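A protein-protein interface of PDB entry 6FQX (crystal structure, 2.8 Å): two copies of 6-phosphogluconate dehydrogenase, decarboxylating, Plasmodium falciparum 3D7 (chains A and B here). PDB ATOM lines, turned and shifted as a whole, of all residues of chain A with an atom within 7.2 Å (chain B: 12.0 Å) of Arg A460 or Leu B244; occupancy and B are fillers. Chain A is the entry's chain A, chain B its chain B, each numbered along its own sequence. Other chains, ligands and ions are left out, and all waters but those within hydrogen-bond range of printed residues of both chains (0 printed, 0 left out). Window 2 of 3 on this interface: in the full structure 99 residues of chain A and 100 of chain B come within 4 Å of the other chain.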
ATOM      1  N   ARG A 456      -3.691  -8.818  13.804  1.00  0.00           N
ATOM      2  CA  ARG A 456      -4.348  -8.376  15.019  1.00  0.00           C
ATOM      3  C   ARG A 456      -5.628  -9.172  15.188  1.00  0.00           C
ATOM      4  O   ARG A 456      -6.096  -9.824  14.250  1.00  0.00           O
ATOM      5  CB  ARG A 456      -4.568  -6.861  14.982  1.00  0.00           C
ATOM      6  CG  ARG A 456      -3.329  -6.203  15.476  1.00  0.00           C
ATOM      7  CD  ARG A 456      -2.905  -5.047  14.667  1.00  0.00           C
ATOM      8  NE  ARG A 456      -2.670  -5.291  13.241  1.00  0.00           N
ATOM      9  CZ  ARG A 456      -1.639  -5.956  12.752  1.00  0.00           C
ATOM     10  NH1 ARG A 456      -0.759  -6.469  13.579  1.00  0.00           N
ATOM     11  NH2 ARG A 456      -1.493  -6.104  11.446  1.00  0.00           N
ATOM     12  N   ARG A 457      -6.143  -9.187  16.414  1.00  0.00           N
ATOM     13  CA  ARG A 457      -7.273 -10.034  16.782  1.00  0.00           C
ATOM     14  C   ARG A 457      -8.536  -9.226  17.055  1.00  0.00           C
ATOM     15  O   ARG A 457      -8.503  -8.005  17.272  1.00  0.00           O
ATOM     16  CB  ARG A 457      -6.960 -10.876  18.026  1.00  0.00           C
ATOM     17  CG  ARG A 457      -5.989 -11.999  17.847  1.00  0.00           C
ATOM     18  CD  ARG A 457      -5.811 -12.683  19.180  1.00  0.00           C
ATOM     19  NE  ARG A 457      -5.559 -14.107  19.068  1.00  0.00           N
ATOM     20  CZ  ARG A 457      -6.459 -15.063  19.295  1.00  0.00           C
ATOM     21  NH1 ARG A 457      -7.692 -14.751  19.674  1.00  0.00           N
ATOM     22  NH2 ARG A 457      -6.109 -16.341  19.160  1.00  0.00           N
ATOM     23  N   THR A 458      -9.665  -9.954  17.051  1.00  0.00           N
ATOM     24  CA  THR A 458     -10.954  -9.358  17.384  1.00  0.00           C
ATOM     25  C   THR A 458     -11.099  -9.142  18.891  1.00  0.00           C
ATOM     26  O   THR A 458     -11.683  -8.136  19.319  1.00  0.00           O
ATOM     27  CB  THR A 458     -12.101 -10.215  16.846  1.00  0.00           C
ATOM     28  OG1 THR A 458     -12.439 -11.232  17.798  1.00  0.00           O
ATOM     29  CG2 THR A 458     -11.697 -10.868  15.547  1.00  0.00           C
ATOM     30  N   ASP A 459     -10.590 -10.079  19.710  1.00  0.00           N
ATOM     31  CA  ASP A 459     -10.807 -10.036  21.154  1.00  0.00           C
ATOM     32  C   ASP A 459      -9.751  -9.271  21.939  1.00  0.00           C
ATOM     33  O   ASP A 459     -10.073  -8.740  23.005  1.00  0.00           O
ATOM     34  CB  ASP A 459     -10.920 -11.452  21.724  1.00  0.00           C
ATOM     35  CG  ASP A 459      -9.822 -12.375  21.251  1.00  0.00           C
ATOM     36  OD1 ASP A 459      -8.925 -11.918  20.520  1.00  0.00           O
ATOM     37  OD2 ASP A 459      -9.830 -13.560  21.656  1.00  0.00           O
ATOM     38  N   ARG A 460      -8.504  -9.201  21.473  1.00  0.00           N
ATOM     39  CA  ARG A 460      -7.430  -8.624  22.281  1.00  0.00           C
ATOM     40  C   ARG A 460      -6.507  -7.755  21.434  1.00  0.00           C
ATOM     41  O   ARG A 460      -6.425  -7.900  20.209  1.00  0.00           O
ATOM     42  CB  ARG A 460      -6.632  -9.724  22.988  1.00  0.00           C
ATOM     43  CG  ARG A 460      -6.115 -10.765  22.049  1.00  0.00           C
ATOM     44  CD  ARG A 460      -6.544 -12.140  22.498  1.00  0.00           C
ATOM     45  NE  ARG A 460      -6.079 -12.413  23.847  1.00  0.00           N
ATOM     46  CZ  ARG A 460      -6.637 -13.284  24.684  1.00  0.00           C
ATOM     47  NH1 ARG A 460      -7.696 -13.997  24.306  1.00  0.00           N
ATOM     48  NH2 ARG A 460      -6.121 -13.444  25.904  1.00  0.00           N
ATOM     49  N   GLU A 461      -5.790  -6.867  22.126  1.00  0.00           N
ATOM     50  CA  GLU A 461      -4.822  -5.937  21.560  1.00  0.00           C
ATOM     51  C   GLU A 461      -3.508  -6.627  21.200  1.00  0.00           C
ATOM     52  O   GLU A 461      -3.148  -7.673  21.740  1.00  0.00           O
ATOM     53  CB  GLU A 461      -4.490  -4.831  22.552  1.00  0.00           C
ATOM     54  CG  GLU A 461      -3.597  -5.314  23.670  1.00  0.00           C
ATOM     55  CD  GLU A 461      -4.349  -5.904  24.837  1.00  0.00           C
ATOM     56  OE1 GLU A 461      -5.578  -6.097  24.723  1.00  0.00           O
ATOM     57  OE2 GLU A 461      -3.694  -6.206  25.858  1.00  0.00           O
ATOM     58  N   GLY A 462      -2.751  -5.972  20.333  1.00  0.00           N
ATOM     59  CA  GLY A 462      -1.380  -6.348  20.060  1.00  0.00           C
ATOM     60  C   GLY A 462      -1.212  -7.125  18.764  1.00  0.00           C
ATOM     61  O   GLY A 462      -2.168  -7.552  18.113  1.00  0.00           O
ATOM     62  N   ASN A 463       0.052  -7.318  18.406  1.00  0.00           N
ATOM     63  CA  ASN A 463       0.413  -8.048  17.203  1.00  0.00           C
ATOM     64  C   ASN A 463       0.664  -9.484  17.590  1.00  0.00           C
ATOM     65  O   ASN A 463       1.224  -9.761  18.654  1.00  0.00           O
ATOM     66  CB  ASN A 463       1.679  -7.485  16.562  1.00  0.00           C
ATOM     67  CG  ASN A 463       1.579  -6.025  16.307  1.00  0.00           C
ATOM     68  OD1 ASN A 463       0.680  -5.577  15.624  1.00  0.00           O
ATOM     69  ND2 ASN A 463       2.438  -5.260  16.936  1.00  0.00           N
ATOM     70  N   TYR A 464       0.261 -10.391  16.718  1.00  0.00           N
ATOM     71  CA  TYR A 464       0.357 -11.806  16.999  1.00  0.00           C
ATOM     72  C   TYR A 464       0.924 -12.487  15.773  1.00  0.00           C
ATOM     73  O   TYR A 464       0.586 -12.121  14.645  1.00  0.00           O
ATOM     74  CB  TYR A 464      -0.993 -12.382  17.354  1.00  0.00           C
ATOM     75  CG  TYR A 464      -1.548 -11.786  18.610  1.00  0.00           C
ATOM     76  CD1 TYR A 464      -2.156 -10.537  18.592  1.00  0.00           C
ATOM     77  CD2 TYR A 464      -1.459 -12.464  19.819  1.00  0.00           C
ATOM     78  CE1 TYR A 464      -2.661  -9.982  19.742  1.00  0.00           C
ATOM     79  CE2 TYR A 464      -1.957 -11.914  20.980  1.00  0.00           C
ATOM     80  CZ  TYR A 464      -2.553 -10.671  20.935  1.00  0.00           C
ATOM     81  OH  TYR A 464      -3.063 -10.116  22.077  1.00  0.00           O
ATOM     82  N   LYS B 240      -6.860 -24.498  10.999  1.00  0.00           N
ATOM     83  CA  LYS B 240      -6.151 -24.247  12.246  1.00  0.00           C
ATOM     84  C   LYS B 240      -7.106 -23.791  13.346  1.00  0.00           C
ATOM     85  O   LYS B 240      -7.937 -22.901  13.131  1.00  0.00           O
ATOM     86  CB  LYS B 240      -5.054 -23.212  12.034  1.00  0.00           C
ATOM     87  CG  LYS B 240      -4.213 -22.923  13.253  1.00  0.00           C
ATOM     88  CD  LYS B 240      -3.028 -23.866  13.419  1.00  0.00           C
ATOM     89  CE  LYS B 240      -2.181 -23.380  14.616  1.00  0.00           C
ATOM     90  NZ  LYS B 240      -0.919 -24.135  14.897  1.00  0.00           N
ATOM     91  N   LYS B 241      -6.959 -24.377  14.540  1.00  0.00           N
ATOM     92  CA  LYS B 241      -7.773 -24.004  15.688  1.00  0.00           C
ATOM     93  C   LYS B 241      -6.987 -23.101  16.631  1.00  0.00           C
ATOM     94  O   LYS B 241      -5.762 -23.202  16.751  1.00  0.00           O
ATOM     95  CB  LYS B 241      -8.286 -25.228  16.473  1.00  0.00           C
ATOM     96  CG  LYS B 241      -9.444 -26.041  15.843  1.00  0.00           C
ATOM     97  CD  LYS B 241     -10.801 -25.536  16.422  1.00  0.00           C
ATOM     98  CE  LYS B 241     -11.971 -26.536  16.342  1.00  0.00           C
ATOM     99  NZ  LYS B 241     -13.303 -25.947  16.823  1.00  0.00           N
ATOM    100  N   ASP B 242      -7.715 -22.205  17.295  1.00  0.00           N
ATOM    101  CA  ASP B 242      -7.106 -21.225  18.182  1.00  0.00           C
ATOM    102  C   ASP B 242      -6.714 -21.904  19.497  1.00  0.00           C
ATOM    103  O   ASP B 242      -7.354 -22.861  19.939  1.00  0.00           O
ATOM    104  CB  ASP B 242      -8.081 -20.066  18.435  1.00  0.00           C
ATOM    105  CG  ASP B 242      -7.430 -18.873  19.126  1.00  0.00           C
ATOM    106  OD1 ASP B 242      -6.239 -18.943  19.479  1.00  0.00           O
ATOM    107  OD2 ASP B 242      -8.106 -17.844  19.343  1.00  0.00           O
ATOM    108  N   ASP B 243      -5.612 -21.445  20.090  1.00  0.00           N
ATOM    109  CA  ASP B 243      -5.243 -21.899  21.429  1.00  0.00           C
ATOM    110  C   ASP B 243      -5.907 -21.071  22.540  1.00  0.00           C
ATOM    111  O   ASP B 243      -6.096 -21.580  23.651  1.00  0.00           O
ATOM    112  CB  ASP B 243      -3.716 -21.923  21.607  1.00  0.00           C
ATOM    113  CG  ASP B 243      -3.026 -20.665  21.089  1.00  0.00           C
ATOM    114  OD1 ASP B 243      -1.784 -20.573  21.250  1.00  0.00           O
ATOM    115  OD2 ASP B 243      -3.695 -19.773  20.517  1.00  0.00           O
ATOM    116  N   LEU B 244      -6.274 -19.815  22.277  1.00  0.00           N
ATOM    117  CA  LEU B 244      -6.834 -18.924  23.288  1.00  0.00           C
ATOM    118  C   LEU B 244      -8.354 -18.901  23.322  1.00  0.00           C
ATOM    119  O   LEU B 244      -8.920 -18.224  24.192  1.00  0.00           O
ATOM    120  CB  LEU B 244      -6.341 -17.500  23.057  1.00  0.00           C
ATOM    121  CG  LEU B 244      -4.843 -17.449  22.821  1.00  0.00           C
ATOM    122  CD1 LEU B 244      -4.307 -16.001  22.668  1.00  0.00           C
ATOM    123  CD2 LEU B 244      -4.191 -18.200  23.960  1.00  0.00           C
ATOM    124  N   THR B 245      -9.011 -19.597  22.395  1.00  0.00           N
ATOM    125  CA  THR B 245     -10.463 -19.711  22.321  1.00  0.00           C
ATOM    126  C   THR B 245     -10.803 -21.092  21.775  1.00  0.00           C
ATOM    127  O   THR B 245      -9.921 -21.850  21.358  1.00  0.00           O
ATOM    128  CB  THR B 245     -11.050 -18.630  21.419  1.00  0.00           C
ATOM    129  OG1 THR B 245     -10.206 -18.495  20.275  1.00  0.00           O
ATOM    130  CG2 THR B 245     -11.114 -17.285  22.129  1.00  0.00           C
ATOM    131  N   ASN B 246     -12.093 -21.423  21.759  1.00  0.00           N
ATOM    132  CA  ASN B 246     -12.515 -22.667  21.130  1.00  0.00           C
ATOM    133  C   ASN B 246     -12.919 -22.477  19.667  1.00  0.00           C
ATOM    134  O   ASN B 246     -13.476 -23.396  19.052  1.00  0.00           O
ATOM    135  CB  ASN B 246     -13.638 -23.323  21.935  1.00  0.00           C
ATOM    136  CG  ASN B 246     -13.109 -24.124  23.111  1.00  0.00           C
ATOM    137  OD1 ASN B 246     -12.077 -24.804  23.006  1.00  0.00           O
ATOM    138  ND2 ASN B 246     -13.811 -24.048  24.241  1.00  0.00           N
ATOM    139  N   ASN B 247     -12.597 -21.327  19.091  1.00  0.00           N
ATOM    140  CA  ASN B 247     -12.892 -21.025  17.702  1.00  0.00           C
ATOM    141  C   ASN B 247     -11.747 -21.458  16.774  1.00  0.00           C
ATOM    142  O   ASN B 247     -10.645 -21.821  17.214  1.00  0.00           O
ATOM    143  CB  ASN B 247     -13.152 -19.529  17.571  1.00  0.00           C
ATOM    144  CG  ASN B 247     -14.339 -19.081  18.399  1.00  0.00           C
ATOM    145  OD1 ASN B 247     -14.162 -18.529  19.489  1.00  0.00           O
ATOM    146  ND2 ASN B 247     -15.550 -19.293  17.887  1.00  0.00           N
ATOM    147  N   TYR B 248     -12.021 -21.392  15.469  1.00  0.00           N
ATOM    148  CA  TYR B 248     -10.978 -21.539  14.460  1.00  0.00           C
ATOM    149  C   TYR B 248     -10.154 -20.252  14.441  1.00  0.00           C
ATOM    150  O   TYR B 248     -10.681 -19.154  14.664  1.00  0.00           O
ATOM    151  CB  TYR B 248     -11.602 -21.810  13.082  1.00  0.00           C
ATOM    152  CG  TYR B 248     -12.203 -23.192  12.964  1.00  0.00           C
ATOM    153  CD1 TYR B 248     -13.541 -23.412  13.269  1.00  0.00           C
ATOM    154  CD2 TYR B 248     -11.425 -24.291  12.634  1.00  0.00           C
ATOM    155  CE1 TYR B 248     -14.100 -24.672  13.211  1.00  0.00           C
ATOM    156  CE2 TYR B 248     -11.983 -25.564  12.560  1.00  0.00           C
ATOM    157  CZ  TYR B 248     -13.317 -25.745  12.851  1.00  0.00           C
ATOM    158  OH  TYR B 248     -13.878 -26.999  12.789  1.00  0.00           O
ATOM    159  N   LEU B 249      -8.839 -20.377  14.218  1.00  0.00           N
ATOM    160  CA  LEU B 249      -8.008 -19.189  14.400  1.00  0.00           C
ATOM    161  C   LEU B 249      -8.347 -18.129  13.368  1.00  0.00           C
ATOM    162  O   LEU B 249      -8.408 -16.943  13.703  1.00  0.00           O
ATOM    163  CB  LEU B 249      -6.519 -19.534  14.354  1.00  0.00           C
ATOM    164  CG  LEU B 249      -5.530 -18.354  14.305  1.00  0.00           C
ATOM    165  CD1 LEU B 249      -5.626 -17.443  15.517  1.00  0.00           C
ATOM    166  CD2 LEU B 249      -4.111 -18.874  14.148  1.00  0.00           C
ATOM    167  N   VAL B 250      -8.661 -18.538  12.134  1.00  0.00           N
ATOM    168  CA  VAL B 250      -8.923 -17.550  11.091  1.00  0.00           C
ATOM    169  C   VAL B 250     -10.113 -16.669  11.454  1.00  0.00           C
ATOM    170  O   VAL B 250     -10.144 -15.485  11.090  1.00  0.00           O
ATOM    171  CB  VAL B 250      -9.117 -18.232   9.719  1.00  0.00           C
ATOM    172  CG1 VAL B 250     -10.515 -18.850   9.568  1.00  0.00           C
ATOM    173  CG2 VAL B 250      -8.814 -17.260   8.631  1.00  0.00           C
ATOM    174  N   ASP B 251     -11.065 -17.193  12.231  1.00  0.00           N
ATOM    175  CA  ASP B 251     -12.225 -16.402  12.626  1.00  0.00           C
ATOM    176  C   ASP B 251     -11.907 -15.392  13.714  1.00  0.00           C
ATOM    177  O   ASP B 251     -12.798 -14.638  14.125  1.00  0.00           O
ATOM    178  CB  ASP B 251     -13.355 -17.310  13.091  1.00  0.00           C
ATOM    179  CG  ASP B 251     -13.941 -18.114  11.965  1.00  0.00           C
ATOM    180  OD1 ASP B 251     -13.561 -17.883  10.797  1.00  0.00           O
ATOM    181  OD2 ASP B 251     -14.806 -18.969  12.239  1.00  0.00           O
ATOM    182  N   MET B 252     -10.680 -15.393  14.223  1.00  0.00           N
ATOM    183  CA  MET B 252     -10.291 -14.466  15.265  1.00  0.00           C
ATOM    184  C   MET B 252      -9.290 -13.432  14.776  1.00  0.00           C
ATOM    185  O   MET B 252      -8.894 -12.553  15.550  1.00  0.00           O
ATOM    186  CB  MET B 252      -9.733 -15.243  16.469  1.00  0.00           C
ATOM    187  CG  MET B 252     -10.646 -16.367  16.931  1.00  0.00           C
ATOM    188  SD  MET B 252     -12.163 -15.834  17.762  1.00  0.00           S
ATOM    189  CE  MET B 252     -11.655 -14.448  18.787  1.00  0.00           C
ATOM    190  N   ILE B 253      -8.908 -13.483  13.501  1.00  0.00           N
ATOM    191  CA  ILE B 253      -8.057 -12.455  12.911  1.00  0.00           C
ATOM    192  C   ILE B 253      -8.922 -11.265  12.503  1.00  0.00           C
ATOM    193  O   ILE B 253     -10.032 -11.419  11.972  1.00  0.00           O
ATOM    194  CB  ILE B 253      -7.267 -13.008  11.701  1.00  0.00           C
ATOM    195  CG1 ILE B 253      -6.152 -13.969  12.116  1.00  0.00           C
ATOM    196  CG2 ILE B 253      -6.607 -11.894  10.924  1.00  0.00           C
ATOM    197  CD1 ILE B 253      -6.512 -15.336  12.391  1.00  0.00           C
ATOM    198  N   LEU B 254      -8.420 -10.063  12.734  1.00  0.00           N
ATOM    199  CA  LEU B 254      -9.188  -8.871  12.440  1.00  0.00           C
ATOM    200  C   LEU B 254      -8.935  -8.484  10.983  1.00  0.00           C
ATOM    201  O   LEU B 254      -7.836  -8.676  10.469  1.00  0.00           O
ATOM    202  CB  LEU B 254      -8.814  -7.744  13.406  1.00  0.00           C
ATOM    203  CG  LEU B 254      -9.264  -6.341  13.038  1.00  0.00           C
ATOM    204  CD1 LEU B 254     -10.772  -6.206  13.318  1.00  0.00           C
ATOM    205  CD2 LEU B 254      -8.484  -5.323  13.836  1.00  0.00           C
ATOM    206  N   ASP B 255      -9.979  -7.993  10.307  1.00  0.00           N
ATOM    207  CA  ASP B 255      -9.992  -7.842   8.841  1.00  0.00           C
ATOM    208  C   ASP B 255      -9.645  -6.412   8.432  1.00  0.00           C
ATOM    209  O   ASP B 255     -10.405  -5.721   7.752  1.00  0.00           O
ATOM    210  CB  ASP B 255     -11.355  -8.246   8.268  1.00  0.00           C
ATOM    211  CG  ASP B 255     -12.506  -7.369   8.789  1.00  0.00           C
ATOM    212  OD1 ASP B 255     -12.431  -6.922   9.951  1.00  0.00           O
ATOM    213  OD2 ASP B 255     -13.494  -7.156   8.045  1.00  0.00           O
ATOM    214  N   ILE B 256      -8.470  -5.960   8.839  1.00  0.00           N
ATOM    215  CA  ILE B 256      -7.960  -4.662   8.418  1.00  0.00           C
ATOM    216  C   ILE B 256      -6.602  -4.974   7.818  1.00  0.00           C
ATOM    217  O   ILE B 256      -5.676  -5.388   8.532  1.00  0.00           O
ATOM    218  CB  ILE B 256      -7.853  -3.668   9.570  1.00  0.00           C
ATOM    219  CG1 ILE B 256      -9.246  -3.455  10.154  1.00  0.00           C
ATOM    220  CG2 ILE B 256      -7.232  -2.357   9.092  1.00  0.00           C
ATOM    221  CD1 ILE B 256      -9.278  -2.502  11.294  1.00  0.00           C
ATOM    222  N   LYS B 293     -12.907   0.220   9.013  1.00  0.00           N
ATOM    223  CA  LYS B 293     -13.798  -0.678   9.748  1.00  0.00           C
ATOM    224  C   LYS B 293     -14.887   0.100  10.488  1.00  0.00           C
ATOM    225  O   LYS B 293     -16.037  -0.344  10.545  1.00  0.00           O
ATOM    226  CB  LYS B 293     -13.029  -1.602  10.714  1.00  0.00           C
ATOM    227  CG  LYS B 293     -13.830  -2.938  10.851  1.00  0.00           C
ATOM    228  CD  LYS B 293     -13.486  -3.811  12.010  1.00  0.00           C
ATOM    229  CE  LYS B 293     -13.928  -5.258  11.781  1.00  0.00           C
ATOM    230  NZ  LYS B 293     -15.351  -5.496  11.438  1.00  0.00           N
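No position is printed for both chains.
Among the printed residues, pairs that only touch across the chains: Arg A457 with Met B252, Asp A459 with Met B252, Arg A456 with Ile B253, Arg A457 with Leu B249, Arg A457 with Leu B254, Arg A460 with Leu B244, Arg A457 with Leu B244, Asp A459 with Thr B245 and Thr A458 with Ile B253.
The side-chain amide oxygen (OD1) of Asn A463 lies within hydrogen-bond range of the guanidinium group (NH1) of Arg A456, 2.7 Å away.
NH1 of Arg A457 lies within salt-bridge range of OD2 of Asp A459 (3.1 Å).
The side-chain carboxylate (OD2) of Asp A459 is in salt-bridge range of the guanidinium group (NH1) of Arg A460, 3.4 Å away.
The backbone carbonyl oxygen (O) of Lys B240 lies within hydrogen-bond range of the backbone NH (N) of Leu B249, 2.9 Å away.
OD1 of Asp B242 is in hydrogen-bond range of N of Leu B244 (2.9 Å).
The side-chain amide oxygen (OD1) of Asn B247 lies close to the side-chain sulfur (SD) of Met B252 (3.8 Å).
O of Arg A456 sits at hydrogen-bond distance from N of Leu B254, 2.8 Å away.
OD2 of Asp B242 lies within salt-bridge range of NH2 of Arg A457 (2.5 Å).
N of Thr A458 is in hydrogen-bond range of O of Met B252 (3.1 Å).
Of the 9 printed residues of chain A, 5 touch a printed residue of chain B.
Of the 18 printed residues of chain B, 7 touch a printed residue of chain A.
Printed residues of chain B that touch a printed residue of chain A: Asp B242, Leu B244, Thr B245, Leu B249, Met B252, Ile B253 and Leu B254.
Hydrophobic or aromatic side chains of chain B that line the printed part of chain A: Leu B244, Leu B249, Met B252, Ile B253 and Leu B254.
Among the printed residues, 12 pairs touch across the chains.
Printed residues of chain B within 4 Å of Arg A456: Ile B253 and Leu B254.
Of chain B, only Asp B242, Leu B244, Leu B249, Met B252 and Leu B254 come within 4 Å of Arg A457.
Printed residues of chain B within 4 Å of Thr A458: Met B252 (3.1 Å) and Ile B253 (3.98 Å).
Of chain B, only Leu B244 (3.96 Å) comes within 4 Å of Arg A460.
No residue of chain B comes within 4 Å of Gly A462.
Lys B241 touches none of the printed residues of chain A.
Of the printed residues of chain A, Asp B242 touches Arg A457 (2.5 Å).
The nearest residue of chain A that does not touch Leu B244 is Tyr A464 (5.0 Å).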
